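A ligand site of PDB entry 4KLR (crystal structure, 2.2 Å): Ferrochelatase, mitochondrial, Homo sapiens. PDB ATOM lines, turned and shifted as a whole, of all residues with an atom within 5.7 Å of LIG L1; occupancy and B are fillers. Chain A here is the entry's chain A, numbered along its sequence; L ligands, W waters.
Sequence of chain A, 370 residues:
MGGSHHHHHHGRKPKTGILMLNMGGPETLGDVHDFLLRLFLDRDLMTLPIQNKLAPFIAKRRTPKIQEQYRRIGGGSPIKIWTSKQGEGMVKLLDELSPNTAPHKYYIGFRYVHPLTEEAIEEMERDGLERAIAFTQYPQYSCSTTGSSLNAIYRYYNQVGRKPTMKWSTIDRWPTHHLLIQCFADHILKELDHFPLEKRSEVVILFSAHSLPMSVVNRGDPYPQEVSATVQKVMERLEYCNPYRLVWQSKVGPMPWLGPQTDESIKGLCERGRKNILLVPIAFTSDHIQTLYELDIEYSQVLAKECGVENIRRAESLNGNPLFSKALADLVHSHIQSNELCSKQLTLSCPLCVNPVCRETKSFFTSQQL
The guanidinium group (NE) of Arg 62 lies within salt-bridge range of an oxygen (O1) of LIG L1 (2.7 Å).
O4 of LIG L1 sits at hydrogen-bond distance from N of Ile 289, at 3.1 Å.
A ring nitrogen (NE2) of His 210 lies within hydrogen-bond range of an oxygen (O3) of LIG L1 (3.5 Å).
An oxygen (O5) of LG2 L2 lies within salt-bridge range of the guanidinium group (NH1) of Arg 62 (3.3 Å).
The side-chain hydroxyl of Tyr 138 is in hydrogen-bond range of the backbone NH of Met 23 (2.9 Å).
The backbone carbonyl oxygen of Val 252 sits at hydrogen-bond distance from the indole nitrogen of Trp 257 (3.0 Å).
The backbone carbonyl oxygen of His 210 sits at hydrogen-bond distance from the side-chain hydroxyl of Tyr 223.
OG of Ser 144 sits at hydrogen-bond distance from OG of Ser 142, at 2.9 Å.
OG1 of Thr 145 lies close to O of Ser 142 (3.5 Å).
Residues that only touch LIG L1: Met 23 (3.2 Å), Leu 36 (3.8 Å), Leu 39 (3.7 Å), Phe 40 (3.5 Å), Leu 45 (3.7 Å), Ile 66 (3.7 Å), Tyr 70 (3.6 Å), Ser 144 (3.5 Å), Thr 145 (3.6 Å), Leu 212 (3.7 Å), Pro 213 (3.7 Å), Tyr 223 (3.8 Å), Val 252 (3.4 Å), Trp 257 (3.8 Å), Ala 283 (3.1 Å), Phe 284 (3.6 Å) and His 288 (3.2 Å).
Hydrophobic or aromatic side chains that line LIG L1: Met 23, Leu 36, Leu 39, Phe 40, Leu 45, Ile 66, His 210, Leu 212, Pro 213, Tyr 223, Val 252, Trp 257, Phe 284, His 288 and Ile 289.
Water W1 lies within hydrogen-bond range of the backbone carbonyl oxygen of Ile 289 (2.7 Å), an oxygen (O3) of LIG L1 (2.7 Å), the side-chain hydroxyl of Ser 250 (2.7 Å) and a ring nitrogen (NE2) of His 210 (3.0 Å).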
ATOM      1  N   MET A  23       1.203 -25.095 -19.996  1.00  0.00           N
ATOM      2  CA  MET A  23       2.038 -25.284 -21.227  1.00  0.00           C
ATOM      3  C   MET A  23       1.199 -25.847 -22.416  1.00  0.00           C
ATOM      4  O   MET A  23       1.615 -25.725 -23.593  1.00  0.00           O
ATOM      5  CB  MET A  23       3.198 -26.244 -21.027  1.00  0.00           C
ATOM      6  CG  MET A  23       2.752 -27.616 -20.386  1.00  0.00           C
ATOM      7  SD  MET A  23       4.205 -28.712 -20.294  1.00  0.00           S
ATOM      8  CE  MET A  23       4.909 -28.040 -18.789  1.00  0.00           C
ATOM      9  N   PHE A  35       3.842 -28.361 -31.005  1.00  0.00           N
ATOM     10  CA  PHE A  35       4.116 -28.383 -29.566  1.00  0.00           C
ATOM     11  C   PHE A  35       5.606 -28.263 -29.264  1.00  0.00           C
ATOM     12  O   PHE A  35       6.014 -27.304 -28.619  1.00  0.00           O
ATOM     13  CB  PHE A  35       3.535 -29.628 -28.908  1.00  0.00           C
ATOM     14  CG  PHE A  35       3.837 -29.748 -27.433  1.00  0.00           C
ATOM     15  CD1 PHE A  35       3.151 -28.961 -26.495  1.00  0.00           C
ATOM     16  CD2 PHE A  35       4.777 -30.671 -26.977  1.00  0.00           C
ATOM     17  CE1 PHE A  35       3.422 -29.066 -25.121  1.00  0.00           C
ATOM     18  CE2 PHE A  35       5.040 -30.794 -25.608  1.00  0.00           C
ATOM     19  CZ  PHE A  35       4.377 -29.999 -24.692  1.00  0.00           C
ATOM     20  N   LEU A  36       6.404 -29.176 -29.785  1.00  0.00           N
ATOM     21  CA  LEU A  36       7.818 -29.191 -29.528  1.00  0.00           C
ATOM     22  C   LEU A  36       8.550 -28.003 -30.117  1.00  0.00           C
ATOM     23  O   LEU A  36       9.523 -27.487 -29.542  1.00  0.00           O
ATOM     24  CB  LEU A  36       8.424 -30.433 -30.108  1.00  0.00           C
ATOM     25  CG  LEU A  36       8.200 -31.749 -29.385  1.00  0.00           C
ATOM     26  CD1 LEU A  36       9.117 -32.790 -30.031  1.00  0.00           C
ATOM     27  CD2 LEU A  36       8.518 -31.554 -27.867  1.00  0.00           C
ATOM     28  N   LEU A  39       8.155 -25.084 -27.984  1.00  0.00           N
ATOM     29  CA  LEU A  39       8.831 -25.357 -26.726  1.00  0.00           C
ATOM     30  C   LEU A  39      10.321 -25.063 -26.859  1.00  0.00           C
ATOM     31  O   LEU A  39      10.887 -24.340 -26.009  1.00  0.00           O
ATOM     32  CB  LEU A  39       8.599 -26.811 -26.284  1.00  0.00           C
ATOM     33  CG  LEU A  39       9.046 -27.187 -24.859  1.00  0.00           C
ATOM     34  CD1 LEU A  39       8.227 -28.408 -24.399  1.00  0.00           C
ATOM     35  CD2 LEU A  39      10.532 -27.495 -24.880  1.00  0.00           C
ATOM     36  N   PHE A  40      10.962 -25.571 -27.912  1.00  0.00           N
ATOM     37  CA  PHE A  40      12.401 -25.321 -28.101  1.00  0.00           C
ATOM     38  C   PHE A  40      12.715 -23.911 -28.590  1.00  0.00           C
ATOM     39  O   PHE A  40      13.847 -23.488 -28.528  1.00  0.00           O
ATOM     40  CB  PHE A  40      13.077 -26.388 -28.967  1.00  0.00           C
ATOM     41  CG  PHE A  40      13.140 -27.749 -28.303  1.00  0.00           C
ATOM     42  CD1 PHE A  40      12.260 -28.760 -28.683  1.00  0.00           C
ATOM     43  CD2 PHE A  40      14.074 -28.009 -27.299  1.00  0.00           C
ATOM     44  CE1 PHE A  40      12.317 -30.022 -28.056  1.00  0.00           C
ATOM     45  CE2 PHE A  40      14.131 -29.258 -26.678  1.00  0.00           C
ATOM     46  CZ  PHE A  40      13.251 -30.269 -27.058  1.00  0.00           C
ATOM     47  N   LEU A  45      12.416 -20.360 -20.242  1.00  0.00           N
ATOM     48  CA  LEU A  45      12.659 -21.797 -20.465  1.00  0.00           C
ATOM     49  C   LEU A  45      14.085 -22.207 -20.780  1.00  0.00           C
ATOM     50  O   LEU A  45      14.685 -22.991 -20.021  1.00  0.00           O
ATOM     51  CB  LEU A  45      11.732 -22.457 -21.520  1.00  0.00           C
ATOM     52  CG  LEU A  45      11.140 -23.874 -21.221  1.00  0.00           C
ATOM     53  CD1 LEU A  45      10.636 -24.690 -22.423  1.00  0.00           C
ATOM     54  CD2 LEU A  45      12.032 -24.742 -20.415  1.00  0.00           C
ATOM     55  N   MET A  46      14.607 -21.802 -21.932  1.00  0.00           N
ATOM     56  CA  MET A  46      15.960 -22.216 -22.294  1.00  0.00           C
ATOM     57  C   MET A  46      16.584 -21.321 -23.356  1.00  0.00           C
ATOM     58  O   MET A  46      15.903 -20.790 -24.216  1.00  0.00           O
ATOM     59  CB  MET A  46      16.030 -23.697 -22.725  1.00  0.00           C
ATOM     60  CG  MET A  46      15.377 -23.979 -24.056  1.00  0.00           C
ATOM     61  SD  MET A  46      15.410 -25.721 -24.543  1.00  0.00           S
ATOM     62  CE  MET A  46      13.870 -26.364 -23.851  1.00  0.00           C
ATOM     63  N   ARG A  62      13.214 -35.048 -32.253  1.00  0.00           N
ATOM     64  CA  ARG A  62      12.624 -35.637 -31.048  1.00  0.00           C
ATOM     65  C   ARG A  62      11.153 -36.053 -31.216  1.00  0.00           C
ATOM     66  O   ARG A  62      10.646 -36.825 -30.394  1.00  0.00           O
ATOM     67  CB  ARG A  62      12.755 -34.672 -29.836  1.00  0.00           C
ATOM     68  CG  ARG A  62      14.075 -34.791 -29.139  1.00  0.00           C
ATOM     69  CD  ARG A  62      14.155 -33.940 -27.875  1.00  0.00           C
ATOM     70  NE  ARG A  62      13.770 -34.620 -26.638  1.00  0.00           N
ATOM     71  CZ  ARG A  62      14.514 -35.537 -26.020  1.00  0.00           C
ATOM     72  NH1 ARG A  62      15.658 -35.916 -26.542  1.00  0.00           N
ATOM     73  NH2 ARG A  62      14.112 -36.092 -24.863  1.00  0.00           N
ATOM     74  N   ILE A  66       8.651 -38.549 -28.836  1.00  0.00           N
ATOM     75  CA  ILE A  66       7.615 -37.978 -28.018  1.00  0.00           C
ATOM     76  C   ILE A  66       6.213 -38.422 -28.497  1.00  0.00           C
ATOM     77  O   ILE A  66       5.308 -38.564 -27.692  1.00  0.00           O
ATOM     78  CB  ILE A  66       7.774 -36.432 -27.950  1.00  0.00           C
ATOM     79  CG1 ILE A  66       9.155 -36.016 -27.370  1.00  0.00           C
ATOM     80  CG2 ILE A  66       6.592 -35.760 -27.260  1.00  0.00           C
ATOM     81  CD1 ILE A  66       9.719 -36.941 -26.289  1.00  0.00           C
ATOM     82  N   TYR A  70       3.463 -40.311 -26.110  1.00  0.00           N
ATOM     83  CA  TYR A  70       2.064 -39.951 -25.951  1.00  0.00           C
ATOM     84  C   TYR A  70       1.224 -41.106 -26.439  1.00  0.00           C
ATOM     85  O   TYR A  70       0.137 -41.304 -25.920  1.00  0.00           O
ATOM     86  CB  TYR A  70       1.678 -38.634 -26.667  1.00  0.00           C
ATOM     87  CG  TYR A  70       1.909 -37.371 -25.841  1.00  0.00           C
ATOM     88  CD1 TYR A  70       3.018 -36.571 -26.101  1.00  0.00           C
ATOM     89  CD2 TYR A  70       1.074 -37.030 -24.777  1.00  0.00           C
ATOM     90  CE1 TYR A  70       3.247 -35.410 -25.349  1.00  0.00           C
ATOM     91  CE2 TYR A  70       1.295 -35.855 -24.025  1.00  0.00           C
ATOM     92  CZ  TYR A  70       2.371 -35.061 -24.345  1.00  0.00           C
ATOM     93  OH  TYR A  70       2.670 -33.938 -23.642  1.00  0.00           O
ATOM     94  N   TYR A 138      -0.212 -24.014 -12.541  1.00  0.00           N
ATOM     95  CA  TYR A 138       0.894 -24.755 -11.842  1.00  0.00           C
ATOM     96  C   TYR A 138       0.852 -24.273 -10.406  1.00  0.00           C
ATOM     97  O   TYR A 138       1.026 -23.074 -10.124  1.00  0.00           O
ATOM     98  CB  TYR A 138       2.224 -24.339 -12.390  1.00  0.00           C
ATOM     99  CG  TYR A 138       2.430 -24.555 -13.872  1.00  0.00           C
ATOM    100  CD1 TYR A 138       2.316 -23.502 -14.771  1.00  0.00           C
ATOM    101  CD2 TYR A 138       2.870 -25.806 -14.366  1.00  0.00           C
ATOM    102  CE1 TYR A 138       2.615 -23.675 -16.174  1.00  0.00           C
ATOM    103  CE2 TYR A 138       3.150 -25.970 -15.728  1.00  0.00           C
ATOM    104  CZ  TYR A 138       2.983 -24.910 -16.617  1.00  0.00           C
ATOM    105  OH  TYR A 138       3.317 -25.075 -17.974  1.00  0.00           O
ATOM    106  N   SER A 142       7.787 -22.151 -10.995  1.00  0.00           N
ATOM    107  CA  SER A 142       9.138 -22.149 -11.557  1.00  0.00           C
ATOM    108  C   SER A 142       9.241 -21.074 -12.630  1.00  0.00           C
ATOM    109  O   SER A 142       8.246 -20.727 -13.260  1.00  0.00           O
ATOM    110  CB  SER A 142       9.409 -23.482 -12.205  1.00  0.00           C
ATOM    111  OG  SER A 142      10.672 -23.453 -12.776  1.00  0.00           O
ATOM    112  N   SER A 144      10.442 -21.557 -15.289  1.00  0.00           N
ATOM    113  CA  SER A 144      10.318 -22.232 -16.566  1.00  0.00           C
ATOM    114  C   SER A 144       8.865 -22.458 -16.905  1.00  0.00           C
ATOM    115  O   SER A 144       8.604 -22.832 -18.013  1.00  0.00           O
ATOM    116  CB  SER A 144      10.979 -23.596 -16.513  1.00  0.00           C
ATOM    117  OG  SER A 144      10.420 -24.369 -15.469  1.00  0.00           O
ATOM    118  N   THR A 145       7.950 -22.302 -15.947  1.00  0.00           N
ATOM    119  CA  THR A 145       6.548 -22.708 -16.178  1.00  0.00           C
ATOM    120  C   THR A 145       5.712 -21.488 -16.029  1.00  0.00           C
ATOM    121  O   THR A 145       5.492 -20.779 -17.020  1.00  0.00           O
ATOM    122  CB  THR A 145       6.025 -23.878 -15.238  1.00  0.00           C
ATOM    123  OG1 THR A 145       6.449 -23.650 -13.895  1.00  0.00           O
ATOM    124  CG2 THR A 145       6.599 -25.203 -15.698  1.00  0.00           C
ATOM    125  N   HIS A 210       8.192 -33.111 -11.762  1.00  0.00           N
ATOM    126  CA  HIS A 210       9.167 -32.983 -12.846  1.00  0.00           C
ATOM    127  C   HIS A 210      10.418 -32.314 -12.316  1.00  0.00           C
ATOM    128  O   HIS A 210      10.322 -31.295 -11.536  1.00  0.00           O
ATOM    129  CB  HIS A 210       8.595 -32.090 -13.963  1.00  0.00           C
ATOM    130  CG  HIS A 210       7.604 -32.784 -14.818  1.00  0.00           C
ATOM    131  ND1 HIS A 210       6.257 -32.835 -14.512  1.00  0.00           N
ATOM    132  CD2 HIS A 210       7.760 -33.504 -15.971  1.00  0.00           C
ATOM    133  CE1 HIS A 210       5.623 -33.545 -15.442  1.00  0.00           C
ATOM    134  NE2 HIS A 210       6.512 -33.948 -16.341  1.00  0.00           N
ATOM    135  N   SER A 211      11.569 -32.838 -12.748  1.00  0.00           N
ATOM    136  CA  SER A 211      12.875 -32.352 -12.329  1.00  0.00           C
ATOM    137  C   SER A 211      13.178 -31.041 -13.026  1.00  0.00           C
ATOM    138  O   SER A 211      12.510 -30.685 -14.006  1.00  0.00           O
ATOM    139  CB  SER A 211      13.975 -33.412 -12.613  1.00  0.00           C
ATOM    140  OG  SER A 211      15.223 -32.976 -12.119  1.00  0.00           O
ATOM    141  N   LEU A 212      14.165 -30.332 -12.493  1.00  0.00           N
ATOM    142  CA  LEU A 212      14.758 -29.170 -13.110  1.00  0.00           C
ATOM    143  C   LEU A 212      16.275 -29.422 -13.225  1.00  0.00           C
ATOM    144  O   LEU A 212      16.832 -30.112 -12.418  1.00  0.00           O
ATOM    145  CB  LEU A 212      14.619 -27.934 -12.196  1.00  0.00           C
ATOM    146  CG  LEU A 212      13.294 -27.251 -11.897  1.00  0.00           C
ATOM    147  CD1 LEU A 212      13.506 -26.117 -10.919  1.00  0.00           C
ATOM    148  CD2 LEU A 212      12.637 -26.775 -13.156  1.00  0.00           C
ATOM    149  N   PRO A 213      16.936 -28.872 -14.251  1.00  0.00           N
ATOM    150  CA  PRO A 213      18.389 -28.954 -14.369  1.00  0.00           C
ATOM    151  C   PRO A 213      19.005 -28.204 -13.217  1.00  0.00           C
ATOM    152  O   PRO A 213      18.490 -27.155 -12.815  1.00  0.00           O
ATOM    153  CB  PRO A 213      18.708 -28.192 -15.653  1.00  0.00           C
ATOM    154  CG  PRO A 213      17.385 -27.946 -16.323  1.00  0.00           C
ATOM    155  CD  PRO A 213      16.355 -27.937 -15.253  1.00  0.00           C
ATOM    156  N   VAL A 216      19.527 -24.603 -13.286  1.00  0.00           N
ATOM    157  CA  VAL A 216      18.361 -23.746 -13.011  1.00  0.00           C
ATOM    158  C   VAL A 216      18.069 -23.659 -11.451  1.00  0.00           C
ATOM    159  O   VAL A 216      17.831 -22.569 -10.906  1.00  0.00           O
ATOM    160  CB  VAL A 216      17.153 -24.168 -13.853  1.00  0.00           C
ATOM    161  CG1 VAL A 216      15.857 -23.462 -13.382  1.00  0.00           C
ATOM    162  CG2 VAL A 216      17.403 -23.765 -15.450  1.00  0.00           C
ATOM    163  N   TYR A 223      10.884 -23.270  -7.351  1.00  0.00           N
ATOM    164  CA  TYR A 223      10.127 -24.493  -7.478  1.00  0.00           C
ATOM    165  C   TYR A 223      10.356 -25.686  -6.515  1.00  0.00           C
ATOM    166  O   TYR A 223       9.406 -26.200  -5.969  1.00  0.00           O
ATOM    167  CB  TYR A 223      10.192 -24.920  -8.952  1.00  0.00           C
ATOM    168  CG  TYR A 223       9.558 -26.233  -9.365  1.00  0.00           C
ATOM    169  CD1 TYR A 223       8.202 -26.317  -9.719  1.00  0.00           C
ATOM    170  CD2 TYR A 223      10.335 -27.374  -9.464  1.00  0.00           C
ATOM    171  CE1 TYR A 223       7.689 -27.521 -10.139  1.00  0.00           C
ATOM    172  CE2 TYR A 223       9.842 -28.559  -9.862  1.00  0.00           C
ATOM    173  CZ  TYR A 223       8.519 -28.636 -10.208  1.00  0.00           C
ATOM    174  OH  TYR A 223       8.088 -29.830 -10.673  1.00  0.00           O
ATOM    175  N   SER A 250      11.425 -37.675 -14.976  1.00  0.00           N
ATOM    176  CA  SER A 250      11.420 -37.370 -16.427  1.00  0.00           C
ATOM    177  C   SER A 250      12.580 -36.455 -16.878  1.00  0.00           C
ATOM    178  O   SER A 250      12.419 -35.742 -17.891  1.00  0.00           O
ATOM    179  CB  SER A 250      10.070 -36.749 -16.869  1.00  0.00           C
ATOM    180  OG  SER A 250       8.922 -37.527 -16.497  1.00  0.00           O
ATOM    181  N   VAL A 252      15.571 -34.924 -18.838  1.00  0.00           N
ATOM    182  CA  VAL A 252      15.926 -34.980 -20.269  1.00  0.00           C
ATOM    183  C   VAL A 252      17.405 -34.615 -20.629  1.00  0.00           C
ATOM    184  O   VAL A 252      18.006 -33.733 -19.988  1.00  0.00           O
ATOM    185  CB  VAL A 252      14.784 -34.354 -21.206  1.00  0.00           C
ATOM    186  CG1 VAL A 252      13.526 -35.251 -21.208  1.00  0.00           C
ATOM    187  CG2 VAL A 252      14.376 -32.967 -20.779  1.00  0.00           C
ATOM    188  N   TRP A 257      20.622 -33.048 -13.449  1.00  0.00           N
ATOM    189  CA  TRP A 257      19.269 -32.560 -13.077  1.00  0.00           C
ATOM    190  C   TRP A 257      19.070 -32.863 -11.613  1.00  0.00           C
ATOM    191  O   TRP A 257      19.756 -33.754 -11.050  1.00  0.00           O
ATOM    192  CB  TRP A 257      18.173 -33.348 -13.875  1.00  0.00           C
ATOM    193  CG  TRP A 257      17.991 -32.814 -15.295  1.00  0.00           C
ATOM    194  CD1 TRP A 257      18.966 -32.816 -16.303  1.00  0.00           C
ATOM    195  CD2 TRP A 257      16.830 -32.210 -15.888  1.00  0.00           C
ATOM    196  NE1 TRP A 257      18.478 -32.217 -17.439  1.00  0.00           N
ATOM    197  CE2 TRP A 257      17.179 -31.843 -17.233  1.00  0.00           C
ATOM    198  CE3 TRP A 257      15.539 -31.922 -15.436  1.00  0.00           C
ATOM    199  CZ2 TRP A 257      16.268 -31.264 -18.131  1.00  0.00           C
ATOM    200  CZ3 TRP A 257      14.640 -31.254 -16.310  1.00  0.00           C
ATOM    201  CH2 TRP A 257      15.004 -30.973 -17.644  1.00  0.00           C
ATOM    202  N   ALA A 283       2.876 -32.045  -8.808  1.00  0.00           N
ATOM    203  CA  ALA A 283       3.294 -30.760  -9.409  1.00  0.00           C
ATOM    204  C   ALA A 283       2.821 -30.502 -10.850  1.00  0.00           C
ATOM    205  O   ALA A 283       3.254 -29.492 -11.484  1.00  0.00           O
ATOM    206  CB  ALA A 283       4.786 -30.534  -9.362  1.00  0.00           C
ATOM    207  N   PHE A 284       1.944 -31.353 -11.344  1.00  0.00           N
ATOM    208  CA  PHE A 284       1.284 -31.137 -12.666  1.00  0.00           C
ATOM    209  C   PHE A 284      -0.072 -31.810 -12.560  1.00  0.00           C
ATOM    210  O   PHE A 284      -0.115 -33.015 -12.315  1.00  0.00           O
ATOM    211  CB  PHE A 284       2.099 -31.665 -13.836  1.00  0.00           C
ATOM    212  CG  PHE A 284       1.721 -31.070 -15.182  1.00  0.00           C
ATOM    213  CD1 PHE A 284       2.132 -29.765 -15.540  1.00  0.00           C
ATOM    214  CD2 PHE A 284       0.933 -31.781 -16.081  1.00  0.00           C
ATOM    215  CE1 PHE A 284       1.772 -29.187 -16.803  1.00  0.00           C
ATOM    216  CE2 PHE A 284       0.570 -31.204 -17.330  1.00  0.00           C
ATOM    217  CZ  PHE A 284       1.018 -29.903 -17.688  1.00  0.00           C
ATOM    218  N   HIS A 288      -0.048 -36.918 -17.777  1.00  0.00           N
ATOM    219  CA  HIS A 288       1.184 -36.635 -18.521  1.00  0.00           C
ATOM    220  C   HIS A 288       2.040 -37.916 -18.675  1.00  0.00           C
ATOM    221  O   HIS A 288       1.657 -38.981 -18.215  1.00  0.00           O
ATOM    222  CB  HIS A 288       2.024 -35.523 -17.813  1.00  0.00           C
ATOM    223  CG  HIS A 288       2.327 -35.812 -16.371  1.00  0.00           C
ATOM    224  ND1 HIS A 288       1.423 -35.576 -15.355  1.00  0.00           N
ATOM    225  CD2 HIS A 288       3.427 -36.366 -15.793  1.00  0.00           C
ATOM    226  CE1 HIS A 288       1.979 -35.929 -14.203  1.00  0.00           C
ATOM    227  NE2 HIS A 288       3.199 -36.386 -14.440  1.00  0.00           N
ATOM    228  N   ILE A 289       3.153 -37.795 -19.376  1.00  0.00           N
ATOM    229  CA  ILE A 289       3.962 -38.941 -19.689  1.00  0.00           C
ATOM    230  C   ILE A 289       4.404 -39.551 -18.390  1.00  0.00           C
ATOM    231  O   ILE A 289       4.788 -38.833 -17.443  1.00  0.00           O
ATOM    232  CB  ILE A 289       5.214 -38.563 -20.539  1.00  0.00           C
ATOM    233  CG1 ILE A 289       4.789 -38.125 -21.934  1.00  0.00           C
ATOM    234  CG2 ILE A 289       6.099 -39.758 -20.731  1.00  0.00           C
ATOM    235  CD1 ILE A 289       5.899 -37.360 -22.684  1.00  0.00           C
HETATM  236  C1  LIG L   1       8.079 -31.377 -21.624  1.00  0.00           C
HETATM  237  C2  LIG L   1      12.401 -29.499 -20.664  1.00  0.00           C
HETATM  238  C3  LIG L   1      10.645 -27.970 -16.446  1.00  0.00           C
HETATM  239  C4  LIG L   1       6.541 -30.171 -17.126  1.00  0.00           C
HETATM  240  C5  LIG L   1       9.374 -30.993 -21.759  1.00  0.00           C
HETATM  241  C6  LIG L   1      10.172 -31.144 -22.948  1.00  0.00           C
HETATM  242  C7  LIG L   1      11.373 -30.645 -22.676  1.00  0.00           C
HETATM  243  C8  LIG L   1      11.362 -30.144 -21.325  1.00  0.00           C
HETATM  244  C9  LIG L   1      12.594 -30.537 -23.589  1.00  0.00           C
HETATM  245  C10 LIG L   1       9.621 -31.791 -24.267  1.00  0.00           C
HETATM  246  C11 LIG L   1       9.749 -33.296 -24.161  1.00  0.00           C
HETATM  247  C12 LIG L   1      11.106 -33.733 -24.612  1.00  0.00           C
HETATM  248  O1  LIG L   1      11.716 -33.201 -25.616  1.00  0.00           O
HETATM  249  O2  LIG L   1      11.595 -34.693 -23.987  1.00  0.00           O
HETATM  250  C13 LIG L   1      12.256 -28.841 -19.460  1.00  0.00           C
HETATM  251  C14 LIG L   1      13.206 -27.904 -18.892  1.00  0.00           C
HETATM  252  C15 LIG L   1      12.694 -27.479 -17.756  1.00  0.00           C
HETATM  253  C16 LIG L   1      11.436 -28.154 -17.533  1.00  0.00           C
HETATM  254  C17 LIG L   1      14.557 -27.446 -19.509  1.00  0.00           C
HETATM  255  C18 LIG L   1      13.369 -26.486 -16.788  1.00  0.00           C
HETATM  256  C19 LIG L   1      13.949 -25.361 -17.186  1.00  0.00           C
HETATM  257  C20 LIG L   1       9.407 -28.442 -16.224  1.00  0.00           C
HETATM  258  C21 LIG L   1       8.584 -28.197 -15.062  1.00  0.00           C
HETATM  259  C22 LIG L   1       7.440 -28.790 -15.226  1.00  0.00           C
HETATM  260  C23 LIG L   1       7.492 -29.451 -16.489  1.00  0.00           C
HETATM  261  C24 LIG L   1       8.870 -27.381 -13.815  1.00  0.00           C
HETATM  262  C25 LIG L   1       6.417 -28.663 -14.062  1.00  0.00           C
HETATM  263  C26 LIG L   1       5.286 -29.258 -13.878  1.00  0.00           C
HETATM  264  C27 LIG L   1       6.628 -30.660 -18.429  1.00  0.00           C
HETATM  265  C28 LIG L   1       5.544 -31.408 -19.049  1.00  0.00           C
HETATM  266  C29 LIG L   1       6.018 -31.772 -20.412  1.00  0.00           C
HETATM  267  C30 LIG L   1       7.334 -31.212 -20.486  1.00  0.00           C
HETATM  268  C31 LIG L   1       4.161 -31.716 -18.402  1.00  0.00           C
HETATM  269  C32 LIG L   1       5.252 -32.562 -21.517  1.00  0.00           C
HETATM  270  C33 LIG L   1       5.780 -34.007 -21.639  1.00  0.00           C
HETATM  271  C34 LIG L   1       5.367 -34.772 -20.413  1.00  0.00           C
HETATM  272  O3  LIG L   1       6.277 -35.086 -19.599  1.00  0.00           O
HETATM  273  O4  LIG L   1       4.174 -35.019 -20.197  1.00  0.00           O
HETATM  274  N1  LIG L   1      10.117 -30.378 -20.804  1.00  0.00           N
HETATM  275  N2  LIG L   1      11.166 -28.989 -18.596  1.00  0.00           N
HETATM  276  N3  LIG L   1       8.689 -29.191 -17.084  1.00  0.00           N
HETATM  277  N4  LIG L   1       7.687 -30.551 -19.305  1.00  0.00           N
HETATM  278 FE1  LIG L   1       9.388 -29.757 -18.939  1.00  0.00          FE
HETATM  279  C1  LG2 L   2      19.977 -27.392 -18.738  1.00  0.00           C
HETATM  280  C2  LG2 L   2      21.479 -27.581 -18.634  1.00  0.00           C
HETATM  281  C3  LG2 L   2      22.188 -26.236 -18.837  1.00  0.00           C
HETATM  282  O1  LG2 L   2      23.607 -26.417 -18.678  1.00  0.00           O
HETATM  283  C4  LG2 L   2      21.835 -25.611 -20.209  1.00  0.00           C
HETATM  284  C5  LG2 L   2      20.312 -25.480 -20.444  1.00  0.00           C
HETATM  285  C6  LG2 L   2      19.975 -24.981 -21.875  1.00  0.00           C
HETATM  286  C7  LG2 L   2      19.838 -26.088 -22.950  1.00  0.00           C
HETATM  287  O2  LG2 L   2      21.158 -26.494 -23.376  1.00  0.00           O
HETATM  288  C8  LG2 L   2      19.009 -27.320 -22.515  1.00  0.00           C
HETATM  289  C9  LG2 L   2      19.477 -27.806 -21.132  1.00  0.00           C
HETATM  290  C10 LG2 L   2      19.466 -26.703 -20.019  1.00  0.00           C
HETATM  291  C11 LG2 L   2      18.831 -29.142 -20.708  1.00  0.00           C
HETATM  292  C12 LG2 L   2      18.718 -30.220 -21.809  1.00  0.00           C
HETATM  293  O3  LG2 L   2      19.973 -30.859 -22.081  1.00  0.00           O
HETATM  294  C13 LG2 L   2      18.170 -29.697 -23.124  1.00  0.00           C
HETATM  295  C14 LG2 L   2      19.040 -28.500 -23.525  1.00  0.00           C
HETATM  296  C15 LG2 L   2      18.621 -28.262 -24.972  1.00  0.00           C
HETATM  297  C16 LG2 L   2      18.388 -29.672 -25.513  1.00  0.00           C
HETATM  298  C17 LG2 L   2      18.363 -30.631 -24.316  1.00  0.00           C
HETATM  299  C18 LG2 L   2      16.689 -29.265 -23.032  1.00  0.00           C
HETATM  300  C19 LG2 L   2      18.091 -26.133 -19.720  1.00  0.00           C
HETATM  301  C20 LG2 L   2      17.410 -31.839 -24.545  1.00  0.00           C
HETATM  302  C21 LG2 L   2      16.807 -32.505 -23.318  1.00  0.00           C
HETATM  303  C22 LG2 L   2      18.138 -32.949 -25.274  1.00  0.00           C
HETATM  304  C23 LG2 L   2      17.649 -33.013 -26.724  1.00  0.00           C
HETATM  305  O4  LG2 L   2      19.564 -34.325 -27.277  1.00  0.00           O
HETATM  306  C24 LG2 L   2      18.390 -34.018 -27.588  1.00  0.00           C
HETATM  307  O5  LG2 L   2      17.803 -34.508 -28.591  1.00  0.00           O
HETATM  308  O   HOH W   1       6.497 -36.752 -17.464  1.00  0.00           O
HETATM  309  O   HOH W   2       9.148 -35.144 -20.298  1.00  0.00           O
